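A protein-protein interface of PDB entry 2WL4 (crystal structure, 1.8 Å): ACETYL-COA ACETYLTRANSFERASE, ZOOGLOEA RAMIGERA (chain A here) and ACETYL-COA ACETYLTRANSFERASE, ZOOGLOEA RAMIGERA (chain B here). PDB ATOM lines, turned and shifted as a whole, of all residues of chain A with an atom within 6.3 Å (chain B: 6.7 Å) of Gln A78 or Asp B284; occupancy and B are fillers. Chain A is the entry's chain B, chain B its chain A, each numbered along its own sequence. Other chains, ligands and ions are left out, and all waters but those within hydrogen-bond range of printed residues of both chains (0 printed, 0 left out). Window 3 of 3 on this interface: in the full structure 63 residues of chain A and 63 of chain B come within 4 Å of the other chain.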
ATOM      1  N   ARG A  68      23.729  17.588  -0.865  1.00  0.00           N
ATOM      2  CA  ARG A  68      23.200  16.241  -1.069  1.00  0.00           C
ATOM      3  C   ARG A  68      21.797  16.283  -1.717  1.00  0.00           C
ATOM      4  O   ARG A  68      21.440  15.435  -2.536  1.00  0.00           O
ATOM      5  CB  ARG A  68      23.211  15.467   0.267  1.00  0.00           C
ATOM      6  CG  ARG A  68      22.558  14.073   0.270  1.00  0.00           C
ATOM      7  CD  ARG A  68      23.389  13.008  -0.437  1.00  0.00           C
ATOM      8  NE  ARG A  68      22.969  11.641  -0.038  1.00  0.00           N
ATOM      9  CZ  ARG A  68      23.608  10.539  -0.397  1.00  0.00           C
ATOM     10  NH1 ARG A  68      24.630  10.627  -1.215  1.00  0.00           N
ATOM     11  NH2 ARG A  68      23.229   9.349   0.060  1.00  0.00           N
ATOM     12  N   MET A  72      21.232  14.311  -5.206  1.00  0.00           N
ATOM     13  CA  MET A  72      20.162  13.321  -5.302  1.00  0.00           C
ATOM     14  C   MET A  72      19.156  13.682  -6.404  1.00  0.00           C
ATOM     15  O   MET A  72      18.775  12.833  -7.209  1.00  0.00           O
ATOM     16  CB  MET A  72      19.512  13.107  -3.934  1.00  0.00           C
ATOM     17  CG  MET A  72      20.483  12.404  -2.960  1.00  0.00           C
ATOM     18  SD  MET A  72      20.695  10.609  -3.236  1.00  0.00           S
ATOM     19  CE  MET A  72      19.264  10.057  -2.315  1.00  0.00           C
ATOM     20  N   VAL A  76      22.534  11.541  -8.967  1.00  0.00           N
ATOM     21  CA  VAL A  76      23.801  10.990  -8.477  1.00  0.00           C
ATOM     22  C   VAL A  76      23.435   9.928  -7.441  1.00  0.00           C
ATOM     23  O   VAL A  76      22.558  10.159  -6.606  1.00  0.00           O
ATOM     24  CB  VAL A  76      24.697  12.098  -7.815  1.00  0.00           C
ATOM     25  CG1 VAL A  76      25.924  11.468  -7.143  1.00  0.00           C
ATOM     26  CG2 VAL A  76      25.119  13.122  -8.896  1.00  0.00           C
ATOM     27  N   PRO A  77      24.115   8.765  -7.481  1.00  0.00           N
ATOM     28  CA  PRO A  77      23.722   7.634  -6.624  1.00  0.00           C
ATOM     29  C   PRO A  77      23.801   7.885  -5.115  1.00  0.00           C
ATOM     30  O   PRO A  77      24.641   8.650  -4.639  1.00  0.00           O
ATOM     31  CB  PRO A  77      24.752   6.564  -6.958  1.00  0.00           C
ATOM     32  CG  PRO A  77      25.227   6.894  -8.321  1.00  0.00           C
ATOM     33  CD  PRO A  77      25.163   8.391  -8.447  1.00  0.00           C
ATOM     34  N   GLN A  78      22.957   7.174  -4.365  1.00  0.00           N
ATOM     35  CA  GLN A  78      22.969   7.265  -2.892  1.00  0.00           C
ATOM     36  C   GLN A  78      24.327   6.856  -2.326  1.00  0.00           C
ATOM     37  O   GLN A  78      24.724   7.291  -1.237  1.00  0.00           O
ATOM     38  CB  GLN A  78      21.860   6.395  -2.288  1.00  0.00           C
ATOM     39  CG  GLN A  78      22.149   4.901  -2.335  1.00  0.00           C
ATOM     40  CD  GLN A  78      20.984   4.087  -1.840  1.00  0.00           C
ATOM     41  OE1 GLN A  78      21.137   2.939  -1.421  1.00  0.00           O
ATOM     42  NE2 GLN A  78      19.808   4.680  -1.877  1.00  0.00           N
ATOM     43  N   GLU A  79      25.056   6.037  -3.075  1.00  0.00           N
ATOM     44  CA  GLU A  79      26.367   5.584  -2.625  1.00  0.00           C
ATOM     45  C   GLU A  79      27.471   6.649  -2.752  1.00  0.00           C
ATOM     46  O   GLU A  79      28.546   6.499  -2.162  1.00  0.00           O
ATOM     47  CB  GLU A  79      26.790   4.332  -3.412  1.00  0.00           C
ATOM     48  CG  GLU A  79      25.917   3.105  -3.181  1.00  0.00           C
ATOM     49  CD  GLU A  79      24.661   3.091  -4.034  1.00  0.00           C
ATOM     50  OE1 GLU A  79      24.502   3.969  -4.928  1.00  0.00           O
ATOM     51  OE2 GLU A  79      23.828   2.179  -3.804  1.00  0.00           O
ATOM     52  N   ALA A  80      27.258   7.672  -3.572  1.00  0.00           N
ATOM     53  CA  ALA A  80      28.223   8.778  -3.606  1.00  0.00           C
ATOM     54  C   ALA A  80      27.968   9.632  -2.368  1.00  0.00           C
ATOM     55  O   ALA A  80      27.048   9.350  -1.580  1.00  0.00           O
ATOM     56  CB  ALA A  80      28.062   9.593  -4.867  1.00  0.00           C
ATOM     57  N   THR A  81      28.740  10.700  -2.201  1.00  0.00           N
ATOM     58  CA  THR A  81      28.575  11.548  -1.026  1.00  0.00           C
ATOM     59  C   THR A  81      28.495  13.013  -1.495  1.00  0.00           C
ATOM     60  O   THR A  81      28.650  13.297  -2.682  1.00  0.00           O
ATOM     61  CB  THR A  81      29.739  11.367  -0.041  1.00  0.00           C
ATOM     62  OG1 THR A  81      30.979  11.575  -0.732  1.00  0.00           O
ATOM     63  CG2 THR A  81      29.711   9.931   0.621  1.00  0.00           C
ATOM     64  N   TYR B 153      12.605  12.228   2.779  1.00  0.00           N
ATOM     65  CA  TYR B 153      11.404  11.560   3.303  1.00  0.00           C
ATOM     66  C   TYR B 153      10.566  12.450   4.218  1.00  0.00           C
ATOM     67  O   TYR B 153       9.404  12.157   4.482  1.00  0.00           O
ATOM     68  CB  TYR B 153      11.749  10.221   3.973  1.00  0.00           C
ATOM     69  CG  TYR B 153      12.203   9.237   2.940  1.00  0.00           C
ATOM     70  CD1 TYR B 153      11.285   8.455   2.245  1.00  0.00           C
ATOM     71  CD2 TYR B 153      13.532   9.184   2.554  1.00  0.00           C
ATOM     72  CE1 TYR B 153      11.695   7.592   1.248  1.00  0.00           C
ATOM     73  CE2 TYR B 153      13.953   8.328   1.557  1.00  0.00           C
ATOM     74  CZ  TYR B 153      13.028   7.538   0.904  1.00  0.00           C
ATOM     75  OH  TYR B 153      13.440   6.679  -0.087  1.00  0.00           O
ATOM     76  N   TYR B 155      10.940  13.050   7.372  1.00  0.00           N
ATOM     77  CA  TYR B 155      10.870  12.650   8.775  1.00  0.00           C
ATOM     78  C   TYR B 155      12.186  12.860   9.532  1.00  0.00           C
ATOM     79  O   TYR B 155      13.214  13.113   8.918  1.00  0.00           O
ATOM     80  CB  TYR B 155      10.302  11.223   8.939  1.00  0.00           C
ATOM     81  CG  TYR B 155      10.903  10.111   8.086  1.00  0.00           C
ATOM     82  CD1 TYR B 155      12.275   9.896   8.028  1.00  0.00           C
ATOM     83  CD2 TYR B 155      10.076   9.241   7.376  1.00  0.00           C
ATOM     84  CE1 TYR B 155      12.809   8.857   7.272  1.00  0.00           C
ATOM     85  CE2 TYR B 155      10.597   8.201   6.623  1.00  0.00           C
ATOM     86  CZ  TYR B 155      11.953   8.010   6.568  1.00  0.00           C
ATOM     87  OH  TYR B 155      12.438   6.967   5.800  1.00  0.00           O
ATOM     88  N   VAL B 281      31.323   7.268   2.455  1.00  0.00           N
ATOM     89  CA  VAL B 281      30.544   6.470   1.502  1.00  0.00           C
ATOM     90  C   VAL B 281      29.064   6.763   1.747  1.00  0.00           C
ATOM     91  O   VAL B 281      28.696   7.106   2.856  1.00  0.00           O
ATOM     92  CB  VAL B 281      30.820   4.951   1.666  1.00  0.00           C
ATOM     93  CG1 VAL B 281      29.935   4.146   0.737  1.00  0.00           C
ATOM     94  CG2 VAL B 281      32.303   4.604   1.323  1.00  0.00           C
ATOM     95  N   GLY B 282      28.224   6.623   0.730  1.00  0.00           N
ATOM     96  CA  GLY B 282      26.811   6.935   0.913  1.00  0.00           C
ATOM     97  C   GLY B 282      26.014   5.658   1.128  1.00  0.00           C
ATOM     98  O   GLY B 282      26.460   4.585   0.744  1.00  0.00           O
ATOM     99  N   VAL B 283      24.827   5.780   1.731  1.00  0.00           N
ATOM    100  CA  VAL B 283      23.890   4.658   1.894  1.00  0.00           C
ATOM    101  C   VAL B 283      22.495   5.218   1.637  1.00  0.00           C
ATOM    102  O   VAL B 283      22.361   6.398   1.320  1.00  0.00           O
ATOM    103  CB  VAL B 283      23.914   4.022   3.324  1.00  0.00           C
ATOM    104  CG1 VAL B 283      25.284   3.333   3.640  1.00  0.00           C
ATOM    105  CG2 VAL B 283      23.627   5.059   4.377  1.00  0.00           C
ATOM    106  N   ASP B 284      21.478   4.368   1.744  1.00  0.00           N
ATOM    107  CA  ASP B 284      20.097   4.813   1.602  1.00  0.00           C
ATOM    108  C   ASP B 284      19.754   5.799   2.719  1.00  0.00           C
ATOM    109  O   ASP B 284      20.003   5.521   3.895  1.00  0.00           O
ATOM    110  CB  ASP B 284      19.168   3.624   1.669  1.00  0.00           C
ATOM    111  CG  ASP B 284      17.757   3.949   1.227  1.00  0.00           C
ATOM    112  OD1 ASP B 284      17.191   4.993   1.627  1.00  0.00           O
ATOM    113  OD2 ASP B 284      17.210   3.137   0.462  1.00  0.00           O
ATOM    114  N   PRO B 285      19.153   6.943   2.365  1.00  0.00           N
ATOM    115  CA  PRO B 285      18.762   7.902   3.399  1.00  0.00           C
ATOM    116  C   PRO B 285      17.842   7.291   4.462  1.00  0.00           C
ATOM    117  O   PRO B 285      17.903   7.719   5.613  1.00  0.00           O
ATOM    118  CB  PRO B 285      18.014   8.987   2.610  1.00  0.00           C
ATOM    119  CG  PRO B 285      18.579   8.887   1.211  1.00  0.00           C
ATOM    120  CD  PRO B 285      18.870   7.434   1.002  1.00  0.00           C
ATOM    121  N   LYS B 286      17.004   6.326   4.085  1.00  0.00           N
ATOM    122  CA  LYS B 286      16.062   5.741   5.034  1.00  0.00           C
ATOM    123  C   LYS B 286      16.747   4.990   6.173  1.00  0.00           C
ATOM    124  O   LYS B 286      16.156   4.798   7.232  1.00  0.00           O
ATOM    125  CB  LYS B 286      15.086   4.795   4.328  1.00  0.00           C
ATOM    126  CG  LYS B 286      14.259   5.459   3.245  1.00  0.00           C
ATOM    127  CD  LYS B 286      13.171   4.526   2.706  1.00  0.00           C
ATOM    128  CE  LYS B 286      13.725   3.517   1.721  1.00  0.00           C
ATOM    129  NZ  LYS B 286      14.616   4.168   0.722  1.00  0.00           N
ATOM    130  N   VAL B 287      17.973   4.530   5.929  1.00  0.00           N
ATOM    131  CA  VAL B 287      18.770   3.887   6.962  1.00  0.00           C
ATOM    132  C   VAL B 287      20.168   4.525   7.112  1.00  0.00           C
ATOM    133  O   VAL B 287      21.181   3.826   7.135  1.00  0.00           O
ATOM    134  CB  VAL B 287      18.882   2.370   6.708  1.00  0.00           C
ATOM    135  CG1 VAL B 287      17.508   1.710   6.830  1.00  0.00           C
ATOM    136  CG2 VAL B 287      19.507   2.095   5.330  1.00  0.00           C
ATOM    137  N   MET B 288      20.202   5.849   7.260  1.00  0.00           N
ATOM    138  CA  MET B 288      21.455   6.614   7.341  1.00  0.00           C
ATOM    139  C   MET B 288      22.421   6.150   8.440  1.00  0.00           C
ATOM    140  O   MET B 288      23.659   6.233   8.283  1.00  0.00           O
ATOM    141  CB  MET B 288      21.169   8.129   7.457  1.00  0.00           C
ATOM    142  CG  MET B 288      20.514   8.557   8.776  1.00  0.00           C
ATOM    143  SD  MET B 288      21.703   8.993  10.066  1.00  0.00           S
ATOM    144  CE  MET B 288      20.687   8.861  11.538  1.00  0.00           C
ATOM    145  N   GLY B 289      21.841   5.632   9.523  1.00  0.00           N
ATOM    146  CA  GLY B 289      22.568   5.102  10.671  1.00  0.00           C
ATOM    147  C   GLY B 289      23.542   3.994  10.299  1.00  0.00           C
ATOM    148  O   GLY B 289      24.483   3.706  11.065  1.00  0.00           O
ATOM    149  N   THR B 290      23.337   3.390   9.130  1.00  0.00           N
ATOM    150  CA  THR B 290      24.212   2.291   8.683  1.00  0.00           C
ATOM    151  C   THR B 290      25.454   2.772   7.939  1.00  0.00           C
ATOM    152  O   THR B 290      26.344   1.981   7.615  1.00  0.00           O
ATOM    153  CB  THR B 290      23.490   1.271   7.779  1.00  0.00           C
ATOM    154  OG1 THR B 290      23.136   1.888   6.533  1.00  0.00           O
ATOM    155  CG2 THR B 290      22.242   0.700   8.478  1.00  0.00           C
ATOM    156  N   GLY B 381      20.867  11.921   5.646  1.00  0.00           N
ATOM    157  CA  GLY B 381      20.830  11.958   4.201  1.00  0.00           C
ATOM    158  C   GLY B 381      21.522  10.751   3.631  1.00  0.00           C
ATOM    159  O   GLY B 381      21.555  10.577   2.426  1.00  0.00           O
ATOM    160  N   GLY B 382      22.050   9.900   4.514  1.00  0.00           N
ATOM    161  CA  GLY B 382      22.589   8.632   4.084  1.00  0.00           C
ATOM    162  C   GLY B 382      24.075   8.640   3.787  1.00  0.00           C
ATOM    163  O   GLY B 382      24.517   8.383   2.669  1.00  0.00           O
ATOM    164  N   MET B 383      24.885   8.873   4.806  1.00  0.00           N
ATOM    165  CA  MET B 383      26.321   8.733   4.590  1.00  0.00           C
ATOM    166  C   MET B 383      27.015   8.219   5.823  1.00  0.00           C
ATOM    167  O   MET B 383      26.427   8.159   6.901  1.00  0.00           O
ATOM    168  CB  MET B 383      26.953  10.063   4.130  1.00  0.00           C
ATOM    169  CG  MET B 383      26.462  10.561   2.753  1.00  0.00           C
ATOM    170  SD  MET B 383      27.050  12.224   2.318  1.00  0.00           S
ATOM    171  CE  MET B 383      25.648  13.232   2.864  1.00  0.00           C
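The backbone carbonyl oxygen of Val B283 sits at hydrogen-bond distance from the guanidinium group of Arg A68, at 3.3 Å.
N of Gly B282 lies within hydrogen-bond range of O of Glu A79 (2.9 Å).
O of Gly B382 is in hydrogen-bond range of NH2 of Arg A68 (3.1 Å).
NE of Arg A68 sits at hydrogen-bond distance from O of Gly B381 (3.0 Å).
The backbone NH (N) of Val B283 sits at hydrogen-bond distance from the backbone carbonyl oxygen (O) of Gln A78 (3.3 Å).
N of Asp B284 lies within hydrogen-bond range of OE1 of Gln A78 (3.5 Å).
O of Gln A78 sits at hydrogen-bond distance from NH2 of Arg A68 (2.9 Å).
N of Val B283 is in hydrogen-bond range of O of Gly B382.
The guanidinium group (NH1) of Arg A68 sits at hydrogen-bond distance from the backbone carbonyl oxygen (O) of Ala A80, 2.8 Å away.
The side-chain amino group of Lys B286 is in salt-bridge range of the side-chain carboxylate of Asp B284, at 2.8 Å.
Met A72 touches Pro B285.
Gly B282 touches Gln A78.
C of Val B281 touches O of Glu A79, 3.95 Å away.
Ala A80 touches Gly B282.
Val B281 touches Thr A81 (C to CG2, 3.4 Å).
CG2 of Thr A81 touches N of Gly B282, at 3.6 Å.
SD of Met B383 touches CB of Thr A81 (3.7 Å).
Of the printed residues of chain B, Met A72 touches Pro B285.
Tyr B155 touches none of the printed residues of chain A.
Of the printed residues of chain A, Gly B282 touches Gln A78 (3.0 Å), Glu A79 (2.9 Å), Ala A80 (3.5 Å) and Thr A81 (3.6 Å).
Of chain A, only Gln A78 comes within 4 Å of Asp B284.
Printed residues of chain A within 4 Å of Pro B285: Met A72.
Val B287 touches none of the printed residues of chain A.
The nearest residue of chain A that does not touch Asp B284 is Arg A68 (5.5 Å).
Printed residues of chain A that touch a printed residue of chain B: Arg A68, Met A72, Gln A78, Glu A79, Ala A80 and Thr A81.
Hydrophobic or aromatic side chains of chain A that line the printed part of chain B: Met A72.
Printed residues of chain B that touch a printed residue of chain A: Val B281, Gly B282, Val B283, Asp B284, Pro B285, Gly B381, Gly B382 and Met B383.
Hydrophobic or aromatic side chains of chain B within 4 Å of the printed part of chain A: Val B281, Pro B285 and Met B383.
Among the printed residues, 13 pairs touch across the chains.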
